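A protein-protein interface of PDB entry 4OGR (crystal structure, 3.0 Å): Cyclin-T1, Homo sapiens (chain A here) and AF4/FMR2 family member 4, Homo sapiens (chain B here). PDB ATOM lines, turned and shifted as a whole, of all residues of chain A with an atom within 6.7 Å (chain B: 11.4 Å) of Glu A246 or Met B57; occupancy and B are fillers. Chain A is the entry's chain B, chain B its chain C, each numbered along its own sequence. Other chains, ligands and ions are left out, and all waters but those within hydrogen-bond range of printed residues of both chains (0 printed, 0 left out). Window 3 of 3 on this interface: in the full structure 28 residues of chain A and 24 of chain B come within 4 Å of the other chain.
The side-chain carboxylate (OE2) of Glu A246 lies within salt-bridge range of the guanidinium group (NH2) of Arg B53 (2.7 Å).
The side-chain carboxylate of Glu A246 lies close to the side-chain sulfur of Met B57, 3.0 Å away.
NH1 of Arg B53 sits close to ND1 of His A239, at 3.0 Å.
NE2 of Gln B55 lies within hydrogen-bond range of O of Trp A207 (3.2 Å).
The indole nitrogen of Trp A207 sits at hydrogen-bond distance from the backbone carbonyl oxygen of Gly B59 (3.2 Å).
Of the 15 printed residues of chain A, 5 touch a printed residue of chain B.
Along chain A the printed residues that touch a printed residue of chain B span positions 207 to 252.
Among the printed residues, 13 pairs touch across the chains.
Among the printed residues, Asp or Glu carboxylates within 4 Å of a Lys or Arg side-chain nitrogen of the other chain: Glu A246 with Arg B53.
Among the printed residues, merely in contact across the chains: Trp A207 with Ile B54 (3.6 Å), Trp A207 with Leu B58 (3.6 Å), Trp A207 with Tyr B61 (3.6 Å), Trp A207 with Met B64 (3.9998 Å), Leu A242 with Ile B54 (3.4 Å), Leu A242 with Met B57 (3.4 Å), Leu A252 with Met B57 (3.6 Å) and Leu A252 with Leu B58 (3.9 Å).
NE of Arg B53 lies within hydrogen-bond range of SD of Met B57, 3.7 Å away.
Met B57 touches three residues of chain A.
Of chain B, only Ile B54 (3.4 Å) and Met B57 (3.4 Å) come within 4 Å of Leu A242.
No residue of chain B comes within 4 Å of Gln A243.
No residue of chain B comes within 4 Å of Leu A245.
Thr A248 touches none of the printed residues of chain B.
Arg A251 touches none of the printed residues of chain B.
Of the printed residues of chain A, Leu B58 touches Trp A207 and Leu A252.
Of the printed residues of chain A, Met B64 touches Trp A207 (3.9998 Å).
The nearest residue of chain B that does not touch Glu A246 is Ile B54 (7.5 Å).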
ATOM      1  N   TRP A 207      -4.822  -7.472 -17.139  1.00  0.00           N
ATOM      2  CA  TRP A 207      -4.659  -6.038 -16.931  1.00  0.00           C
ATOM      3  C   TRP A 207      -3.294  -5.556 -17.423  1.00  0.00           C
ATOM      4  O   TRP A 207      -3.200  -4.580 -18.167  1.00  0.00           O
ATOM      5  CB  TRP A 207      -4.831  -5.696 -15.449  1.00  0.00           C
ATOM      6  CG  TRP A 207      -4.813  -4.226 -15.153  1.00  0.00           C
ATOM      7  CD1 TRP A 207      -5.024  -3.208 -16.038  1.00  0.00           C
ATOM      8  CD2 TRP A 207      -4.570  -3.608 -13.883  1.00  0.00           C
ATOM      9  NE1 TRP A 207      -4.928  -1.996 -15.398  1.00  0.00           N
ATOM     10  CE2 TRP A 207      -4.650  -2.214 -14.075  1.00  0.00           C
ATOM     11  CE3 TRP A 207      -4.293  -4.098 -12.605  1.00  0.00           C
ATOM     12  CZ2 TRP A 207      -4.463  -1.306 -13.036  1.00  0.00           C
ATOM     13  CZ3 TRP A 207      -4.106  -3.195 -11.575  1.00  0.00           C
ATOM     14  CH2 TRP A 207      -4.193  -1.814 -11.797  1.00  0.00           C
ATOM     15  N   HIS A 239     -14.650 -12.046 -14.683  1.00  0.00           N
ATOM     16  CA  HIS A 239     -15.812 -11.266 -15.080  1.00  0.00           C
ATOM     17  C   HIS A 239     -16.586 -10.808 -13.849  1.00  0.00           C
ATOM     18  O   HIS A 239     -16.859  -9.620 -13.675  1.00  0.00           O
ATOM     19  CB  HIS A 239     -16.712 -12.100 -15.995  1.00  0.00           C
ATOM     20  CG  HIS A 239     -17.715 -11.301 -16.765  1.00  0.00           C
ATOM     21  ND1 HIS A 239     -17.446 -10.768 -18.009  1.00  0.00           N
ATOM     22  CD2 HIS A 239     -18.990 -10.949 -16.474  1.00  0.00           C
ATOM     23  CE1 HIS A 239     -18.513 -10.126 -18.450  1.00  0.00           C
ATOM     24  NE2 HIS A 239     -19.462 -10.218 -17.536  1.00  0.00           N
ATOM     25  N   PHE A 241     -15.619 -10.717 -10.820  1.00  0.00           N
ATOM     26  CA  PHE A 241     -14.767  -9.917  -9.948  1.00  0.00           C
ATOM     27  C   PHE A 241     -14.849  -8.457 -10.394  1.00  0.00           C
ATOM     28  O   PHE A 241     -15.014  -7.548  -9.580  1.00  0.00           O
ATOM     29  CB  PHE A 241     -13.327 -10.441  -9.993  1.00  0.00           C
ATOM     30  CG  PHE A 241     -12.451  -9.967  -8.857  1.00  0.00           C
ATOM     31  CD1 PHE A 241     -12.868  -8.979  -7.980  1.00  0.00           C
ATOM     32  CD2 PHE A 241     -11.207 -10.542  -8.658  1.00  0.00           C
ATOM     33  CE1 PHE A 241     -12.058  -8.564  -6.944  1.00  0.00           C
ATOM     34  CE2 PHE A 241     -10.394 -10.132  -7.621  1.00  0.00           C
ATOM     35  CZ  PHE A 241     -10.821  -9.144  -6.762  1.00  0.00           C
ATOM     36  N   LEU A 242     -14.740  -8.246 -11.701  1.00  0.00           N
ATOM     37  CA  LEU A 242     -14.824  -6.909 -12.278  1.00  0.00           C
ATOM     38  C   LEU A 242     -16.206  -6.310 -12.045  1.00  0.00           C
ATOM     39  O   LEU A 242     -16.339  -5.115 -11.793  1.00  0.00           O
ATOM     40  CB  LEU A 242     -14.526  -6.952 -13.769  1.00  0.00           C
ATOM     41  CG  LEU A 242     -13.093  -7.371 -14.112  1.00  0.00           C
ATOM     42  CD1 LEU A 242     -13.008  -7.768 -15.585  1.00  0.00           C
ATOM     43  CD2 LEU A 242     -12.057  -6.309 -13.744  1.00  0.00           C
ATOM     44  N   GLN A 243     -17.231  -7.151 -12.143  1.00  0.00           N
ATOM     45  CA  GLN A 243     -18.606  -6.725 -11.914  1.00  0.00           C
ATOM     46  C   GLN A 243     -18.794  -6.162 -10.514  1.00  0.00           C
ATOM     47  O   GLN A 243     -19.496  -5.169 -10.317  1.00  0.00           O
ATOM     48  CB  GLN A 243     -19.559  -7.905 -12.105  1.00  0.00           C
ATOM     49  CG  GLN A 243     -21.028  -7.528 -12.146  1.00  0.00           C
ATOM     50  CD  GLN A 243     -21.918  -8.700 -12.514  1.00  0.00           C
ATOM     51  OE1 GLN A 243     -21.432  -9.793 -12.811  1.00  0.00           O
ATOM     52  NE2 GLN A 243     -23.229  -8.498 -12.429  1.00  0.00           N
ATOM     53  N   ILE A 244     -18.153  -6.806  -9.547  1.00  0.00           N
ATOM     54  CA  ILE A 244     -18.184  -6.357  -8.162  1.00  0.00           C
ATOM     55  C   ILE A 244     -17.408  -5.056  -7.997  1.00  0.00           C
ATOM     56  O   ILE A 244     -17.759  -4.213  -7.176  1.00  0.00           O
ATOM     57  CB  ILE A 244     -17.617  -7.450  -7.225  1.00  0.00           C
ATOM     58  CG1 ILE A 244     -18.618  -8.606  -7.133  1.00  0.00           C
ATOM     59  CG2 ILE A 244     -17.296  -6.884  -5.841  1.00  0.00           C
ATOM     60  CD1 ILE A 244     -18.179  -9.765  -6.266  1.00  0.00           C
ATOM     61  N   LEU A 245     -16.349  -4.901  -8.782  1.00  0.00           N
ATOM     62  CA  LEU A 245     -15.507  -3.717  -8.697  1.00  0.00           C
ATOM     63  C   LEU A 245     -16.252  -2.472  -9.171  1.00  0.00           C
ATOM     64  O   LEU A 245     -16.094  -1.393  -8.602  1.00  0.00           O
ATOM     65  CB  LEU A 245     -14.235  -3.915  -9.520  1.00  0.00           C
ATOM     66  CG  LEU A 245     -13.005  -4.322  -8.709  1.00  0.00           C
ATOM     67  CD1 LEU A 245     -11.900  -4.828  -9.624  1.00  0.00           C
ATOM     68  CD2 LEU A 245     -12.514  -3.159  -7.861  1.00  0.00           C
ATOM     69  N   GLU A 246     -17.054  -2.625 -10.221  1.00  0.00           N
ATOM     70  CA  GLU A 246     -17.837  -1.517 -10.751  1.00  0.00           C
ATOM     71  C   GLU A 246     -18.884  -1.034  -9.756  1.00  0.00           C
ATOM     72  O   GLU A 246     -19.125   0.167  -9.631  1.00  0.00           O
ATOM     73  CB  GLU A 246     -18.535  -1.932 -12.047  1.00  0.00           C
ATOM     74  CG  GLU A 246     -17.601  -2.385 -13.155  1.00  0.00           C
ATOM     75  CD  GLU A 246     -18.326  -3.154 -14.248  1.00  0.00           C
ATOM     76  OE1 GLU A 246     -19.554  -3.350 -14.128  1.00  0.00           O
ATOM     77  OE2 GLU A 246     -17.666  -3.578 -15.222  1.00  0.00           O
ATOM     78  N   LYS A 247     -19.495  -1.972  -9.039  1.00  0.00           N
ATOM     79  CA  LYS A 247     -20.595  -1.646  -8.139  1.00  0.00           C
ATOM     80  C   LYS A 247     -20.129  -0.966  -6.858  1.00  0.00           C
ATOM     81  O   LYS A 247     -20.951  -0.516  -6.059  1.00  0.00           O
ATOM     82  CB  LYS A 247     -21.386  -2.904  -7.779  1.00  0.00           C
ATOM     83  CG  LYS A 247     -22.222  -3.480  -8.912  1.00  0.00           C
ATOM     84  CD  LYS A 247     -23.323  -4.402  -8.383  1.00  0.00           C
ATOM     85  CE  LYS A 247     -22.794  -5.416  -7.366  1.00  0.00           C
ATOM     86  NZ  LYS A 247     -23.852  -6.362  -6.904  1.00  0.00           N
ATOM     87  N   THR A 248     -18.818  -0.887  -6.659  1.00  0.00           N
ATOM     88  CA  THR A 248     -18.276  -0.188  -5.503  1.00  0.00           C
ATOM     89  C   THR A 248     -18.650   1.275  -5.637  1.00  0.00           C
ATOM     90  O   THR A 248     -18.913   1.741  -6.747  1.00  0.00           O
ATOM     91  CB  THR A 248     -16.743  -0.308  -5.406  1.00  0.00           C
ATOM     92  OG1 THR A 248     -16.135   0.241  -6.581  1.00  0.00           O
ATOM     93  CG2 THR A 248     -16.320  -1.759  -5.236  1.00  0.00           C
ATOM     94  N   PRO A 249     -18.693   2.014  -4.517  1.00  0.00           N
ATOM     95  CA  PRO A 249     -18.928   3.446  -4.721  1.00  0.00           C
ATOM     96  C   PRO A 249     -17.729   4.050  -5.447  1.00  0.00           C
ATOM     97  O   PRO A 249     -16.745   3.342  -5.657  1.00  0.00           O
ATOM     98  CB  PRO A 249     -19.085   3.990  -3.298  1.00  0.00           C
ATOM     99  CG  PRO A 249     -18.350   3.027  -2.446  1.00  0.00           C
ATOM    100  CD  PRO A 249     -18.507   1.678  -3.096  1.00  0.00           C
ATOM    101  N   ASN A 250     -17.815   5.310  -5.854  1.00  0.00           N
ATOM    102  CA  ASN A 250     -16.802   5.906  -6.725  1.00  0.00           C
ATOM    103  C   ASN A 250     -16.696   5.160  -8.061  1.00  0.00           C
ATOM    104  O   ASN A 250     -15.803   5.453  -8.857  1.00  0.00           O
ATOM    105  CB  ASN A 250     -15.426   5.920  -6.039  1.00  0.00           C
ATOM    106  CG  ASN A 250     -15.265   7.066  -5.064  1.00  0.00           C
ATOM    107  OD1 ASN A 250     -16.010   8.045  -5.097  1.00  0.00           O
ATOM    108  ND2 ASN A 250     -14.282   6.947  -4.183  1.00  0.00           N
ATOM    109  N   ARG A 251     -17.637   4.242  -8.301  1.00  0.00           N
ATOM    110  CA  ARG A 251     -17.597   3.246  -9.387  1.00  0.00           C
ATOM    111  C   ARG A 251     -16.348   3.287 -10.279  1.00  0.00           C
ATOM    112  O   ARG A 251     -16.437   3.543 -11.481  1.00  0.00           O
ATOM    113  CB  ARG A 251     -18.848   3.387 -10.266  1.00  0.00           C
ATOM    114  CG  ARG A 251     -20.163   3.280  -9.496  1.00  0.00           C
ATOM    115  CD  ARG A 251     -21.281   2.728 -10.363  1.00  0.00           C
ATOM    116  N   LEU A 252     -15.192   3.053  -9.656  1.00  0.00           N
ATOM    117  CA  LEU A 252     -13.899   2.912 -10.341  1.00  0.00           C
ATOM    118  C   LEU A 252     -13.321   4.214 -10.920  1.00  0.00           C
ATOM    119  O   LEU A 252     -12.173   4.226 -11.367  1.00  0.00           O
ATOM    120  CB  LEU A 252     -13.989   1.852 -11.448  1.00  0.00           C
ATOM    121  CG  LEU A 252     -13.837   0.390 -11.003  1.00  0.00           C
ATOM    122  CD1 LEU A 252     -13.844  -0.528 -12.204  1.00  0.00           C
ATOM    123  CD2 LEU A 252     -12.577   0.150 -10.183  1.00  0.00           C
ATOM    124  N   LYS A 253     -14.102   5.292 -10.946  1.00  0.00           N
ATOM    125  CA  LYS A 253     -13.631   6.553 -11.525  1.00  0.00           C
ATOM    126  C   LYS A 253     -12.377   7.062 -10.807  1.00  0.00           C
ATOM    127  O   LYS A 253     -12.266   6.959  -9.586  1.00  0.00           O
ATOM    128  CB  LYS A 253     -14.733   7.614 -11.463  1.00  0.00           C
ATOM    129  N   GLU B  47      -5.896  -8.810 -28.846  1.00  0.00           N
ATOM    130  CA  GLU B  47      -6.611  -8.433 -27.634  1.00  0.00           C
ATOM    131  C   GLU B  47      -7.912  -9.216 -27.518  1.00  0.00           C
ATOM    132  O   GLU B  47      -8.580  -9.476 -28.520  1.00  0.00           O
ATOM    133  CB  GLU B  47      -6.902  -6.930 -27.627  1.00  0.00           C
ATOM    134  CG  GLU B  47      -5.706  -6.061 -27.269  1.00  0.00           C
ATOM    135  CD  GLU B  47      -5.269  -6.238 -25.826  1.00  0.00           C
ATOM    136  OE1 GLU B  47      -5.880  -5.608 -24.936  1.00  0.00           O
ATOM    137  OE2 GLU B  47      -4.315  -7.008 -25.580  1.00  0.00           O
ATOM    138  N   ASP B  48      -8.257  -9.594 -26.291  1.00  0.00           N
ATOM    139  CA  ASP B  48      -9.514 -10.277 -26.011  1.00  0.00           C
ATOM    140  C   ASP B  48     -10.445  -9.336 -25.255  1.00  0.00           C
ATOM    141  O   ASP B  48     -10.001  -8.335 -24.692  1.00  0.00           O
ATOM    142  CB  ASP B  48      -9.267 -11.559 -25.211  1.00  0.00           C
ATOM    143  CG  ASP B  48      -8.696 -11.288 -23.831  1.00  0.00           C
ATOM    144  OD1 ASP B  48      -7.910 -10.329 -23.691  1.00  0.00           O
ATOM    145  OD2 ASP B  48      -9.031 -12.036 -22.887  1.00  0.00           O
ATOM    146  N   LYS B  49     -11.734  -9.662 -25.246  1.00  0.00           N
ATOM    147  CA  LYS B  49     -12.743  -8.794 -24.647  1.00  0.00           C
ATOM    148  C   LYS B  49     -12.502  -8.574 -23.154  1.00  0.00           C
ATOM    149  O   LYS B  49     -12.742  -7.482 -22.635  1.00  0.00           O
ATOM    150  CB  LYS B  49     -14.140  -9.382 -24.865  1.00  0.00           C
ATOM    151  N   LEU B  50     -12.022  -9.610 -22.474  1.00  0.00           N
ATOM    152  CA  LEU B  50     -11.772  -9.543 -21.037  1.00  0.00           C
ATOM    153  C   LEU B  50     -10.730  -8.480 -20.707  1.00  0.00           C
ATOM    154  O   LEU B  50     -10.977  -7.595 -19.890  1.00  0.00           O
ATOM    155  CB  LEU B  50     -11.317 -10.903 -20.508  1.00  0.00           C
ATOM    156  N   SER B  51      -9.564  -8.582 -21.340  1.00  0.00           N
ATOM    157  CA  SER B  51      -8.491  -7.610 -21.151  1.00  0.00           C
ATOM    158  C   SER B  51      -8.975  -6.199 -21.458  1.00  0.00           C
ATOM    159  O   SER B  51      -8.863  -5.303 -20.621  1.00  0.00           O
ATOM    160  CB  SER B  51      -7.293  -7.950 -22.037  1.00  0.00           C
ATOM    161  OG  SER B  51      -6.923  -9.310 -21.893  1.00  0.00           O
ATOM    162  N   SER B  52      -9.507  -6.017 -22.665  1.00  0.00           N
ATOM    163  CA  SER B  52     -10.027  -4.726 -23.110  1.00  0.00           C
ATOM    164  C   SER B  52     -10.930  -4.099 -22.060  1.00  0.00           C
ATOM    165  O   SER B  52     -10.804  -2.914 -21.747  1.00  0.00           O
ATOM    166  CB  SER B  52     -10.800  -4.880 -24.421  1.00  0.00           C
ATOM    167  OG  SER B  52      -9.939  -5.255 -25.482  1.00  0.00           O
ATOM    168  N   ARG B  53     -11.851  -4.898 -21.531  1.00  0.00           N
ATOM    169  CA  ARG B  53     -12.732  -4.442 -20.470  1.00  0.00           C
ATOM    170  C   ARG B  53     -11.904  -3.935 -19.289  1.00  0.00           C
ATOM    171  O   ARG B  53     -11.923  -2.745 -18.986  1.00  0.00           O
ATOM    172  CB  ARG B  53     -13.668  -5.569 -20.020  1.00  0.00           C
ATOM    173  CG  ARG B  53     -14.761  -5.109 -19.068  1.00  0.00           C
ATOM    174  CD  ARG B  53     -15.594  -6.263 -18.533  1.00  0.00           C
ATOM    175  NE  ARG B  53     -16.586  -5.804 -17.562  1.00  0.00           N
ATOM    176  CZ  ARG B  53     -17.349  -6.609 -16.829  1.00  0.00           C
ATOM    177  NH1 ARG B  53     -17.235  -7.925 -16.944  1.00  0.00           N
ATOM    178  NH2 ARG B  53     -18.224  -6.098 -15.971  1.00  0.00           N
ATOM    179  N   ILE B  54     -11.148  -4.840 -18.667  1.00  0.00           N
ATOM    180  CA  ILE B  54     -10.319  -4.534 -17.495  1.00  0.00           C
ATOM    181  C   ILE B  54      -9.559  -3.215 -17.622  1.00  0.00           C
ATOM    182  O   ILE B  54      -9.580  -2.387 -16.709  1.00  0.00           O
ATOM    183  CB  ILE B  54      -9.296  -5.666 -17.230  1.00  0.00           C
ATOM    184  CG1 ILE B  54     -10.016  -6.981 -16.937  1.00  0.00           C
ATOM    185  CG2 ILE B  54      -8.401  -5.337 -16.039  1.00  0.00           C
ATOM    186  CD1 ILE B  54      -9.172  -8.210 -17.173  1.00  0.00           C
ATOM    187  N   GLN B  55      -8.885  -3.031 -18.751  1.00  0.00           N
ATOM    188  CA  GLN B  55      -8.060  -1.849 -18.967  1.00  0.00           C
ATOM    189  C   GLN B  55      -8.909  -0.578 -19.007  1.00  0.00           C
ATOM    190  O   GLN B  55      -8.468   0.486 -18.571  1.00  0.00           O
ATOM    191  CB  GLN B  55      -7.262  -1.990 -20.265  1.00  0.00           C
ATOM    192  CG  GLN B  55      -6.581  -3.351 -20.430  1.00  0.00           C
ATOM    193  CD  GLN B  55      -5.104  -3.272 -20.787  1.00  0.00           C
ATOM    194  OE1 GLN B  55      -4.501  -2.197 -20.805  1.00  0.00           O
ATOM    195  NE2 GLN B  55      -4.512  -4.426 -21.069  1.00  0.00           N
ATOM    196  N   SER B  56     -10.124  -0.695 -19.533  1.00  0.00           N
ATOM    197  CA  SER B  56     -11.047   0.435 -19.608  1.00  0.00           C
ATOM    198  C   SER B  56     -11.526   0.869 -18.224  1.00  0.00           C
ATOM    199  O   SER B  56     -11.897   2.023 -18.016  1.00  0.00           O
ATOM    200  CB  SER B  56     -12.248   0.076 -20.485  1.00  0.00           C
ATOM    201  N   MET B  57     -11.508  -0.071 -17.288  1.00  0.00           N
ATOM    202  CA  MET B  57     -12.044   0.125 -15.944  1.00  0.00           C
ATOM    203  C   MET B  57     -10.985   0.454 -14.891  1.00  0.00           C
ATOM    204  O   MET B  57     -11.176   1.359 -14.080  1.00  0.00           O
ATOM    205  CB  MET B  57     -12.809  -1.134 -15.564  1.00  0.00           C
ATOM    206  CG  MET B  57     -13.805  -1.532 -16.638  1.00  0.00           C
ATOM    207  SD  MET B  57     -14.901  -2.867 -16.173  1.00  0.00           S
ATOM    208  CE  MET B  57     -13.646  -4.103 -15.848  1.00  0.00           C
ATOM    209  N   LEU B  58      -9.879  -0.282 -14.899  1.00  0.00           N
ATOM    210  CA  LEU B  58      -8.794  -0.043 -13.949  1.00  0.00           C
ATOM    211  C   LEU B  58      -7.783   0.957 -14.508  1.00  0.00           C
ATOM    212  O   LEU B  58      -6.973   1.515 -13.767  1.00  0.00           O
ATOM    213  CB  LEU B  58      -8.100  -1.356 -13.586  1.00  0.00           C
ATOM    214  CG  LEU B  58      -8.996  -2.430 -12.967  1.00  0.00           C
ATOM    215  CD1 LEU B  58      -8.226  -3.723 -12.755  1.00  0.00           C
ATOM    216  CD2 LEU B  58      -9.564  -1.934 -11.642  1.00  0.00           C
ATOM    217  N   GLY B  59      -7.841   1.176 -15.817  1.00  0.00           N
ATOM    218  CA  GLY B  59      -6.978   2.138 -16.477  1.00  0.00           C
ATOM    219  C   GLY B  59      -5.735   1.489 -17.054  1.00  0.00           C
ATOM    220  O   GLY B  59      -5.758   0.321 -17.445  1.00  0.00           O
ATOM    221  N   ASN B  60      -4.642   2.245 -17.088  1.00  0.00           N
ATOM    222  CA  ASN B  60      -3.391   1.769 -17.663  1.00  0.00           C
ATOM    223  C   ASN B  60      -2.503   1.183 -16.575  1.00  0.00           C
ATOM    224  O   ASN B  60      -2.140   1.871 -15.622  1.00  0.00           O
ATOM    225  CB  ASN B  60      -2.671   2.907 -18.393  1.00  0.00           C
ATOM    226  CG  ASN B  60      -1.357   2.468 -19.010  1.00  0.00           C
ATOM    227  OD1 ASN B  60      -1.129   1.282 -19.244  1.00  0.00           O
ATOM    228  ND2 ASN B  60      -0.485   3.430 -19.285  1.00  0.00           N
ATOM    229  N   TYR B  61      -2.164  -0.095 -16.718  1.00  0.00           N
ATOM    230  CA  TYR B  61      -1.444  -0.817 -15.678  1.00  0.00           C
ATOM    231  C   TYR B  61      -0.096  -0.186 -15.336  1.00  0.00           C
ATOM    232  O   TYR B  61       0.235  -0.030 -14.164  1.00  0.00           O
ATOM    233  CB  TYR B  61      -1.229  -2.271 -16.093  1.00  0.00           C
ATOM    234  CG  TYR B  61      -0.372  -3.042 -15.116  1.00  0.00           C
ATOM    235  CD1 TYR B  61      -0.894  -3.492 -13.910  1.00  0.00           C
ATOM    236  CD2 TYR B  61       0.960  -3.312 -15.396  1.00  0.00           C
ATOM    237  CE1 TYR B  61      -0.115  -4.193 -13.013  1.00  0.00           C
ATOM    238  CE2 TYR B  61       1.748  -4.012 -14.504  1.00  0.00           C
ATOM    239  CZ  TYR B  61       1.205  -4.450 -13.314  1.00  0.00           C
ATOM    240  OH  TYR B  61       1.987  -5.148 -12.424  1.00  0.00           O
ATOM    241  N   GLU B  63       0.943   2.722 -15.475  1.00  0.00           N
ATOM    242  CA  GLU B  63       0.788   3.964 -14.727  1.00  0.00           C
ATOM    243  C   GLU B  63       0.574   3.704 -13.235  1.00  0.00           C
ATOM    244  O   GLU B  63       0.744   4.604 -12.414  1.00  0.00           O
ATOM    245  CB  GLU B  63      -0.385   4.776 -15.279  1.00  0.00           C
ATOM    246  CG  GLU B  63      -0.013   5.740 -16.391  1.00  0.00           C
ATOM    247  CD  GLU B  63      -1.172   6.031 -17.328  1.00  0.00           C
ATOM    248  OE1 GLU B  63      -2.334   5.987 -16.871  1.00  0.00           O
ATOM    249  OE2 GLU B  63      -0.918   6.311 -18.520  1.00  0.00           O
ATOM    250  N   MET B  64       0.206   2.469 -12.895  1.00  0.00           N
ATOM    251  CA  MET B  64      -0.191   2.111 -11.531  1.00  0.00           C
ATOM    252  C   MET B  64       0.802   1.173 -10.848  1.00  0.00           C
ATOM    253  O   MET B  64       0.913   1.162  -9.622  1.00  0.00           O
ATOM    254  CB  MET B  64      -1.572   1.445 -11.539  1.00  0.00           C
ATOM    255  CG  MET B  64      -2.637   2.184 -12.340  1.00  0.00           C
ATOM    256  SD  MET B  64      -3.291   3.646 -11.512  1.00  0.00           S
ATOM    257  CE  MET B  64      -5.005   3.541 -12.020  1.00  0.00           C
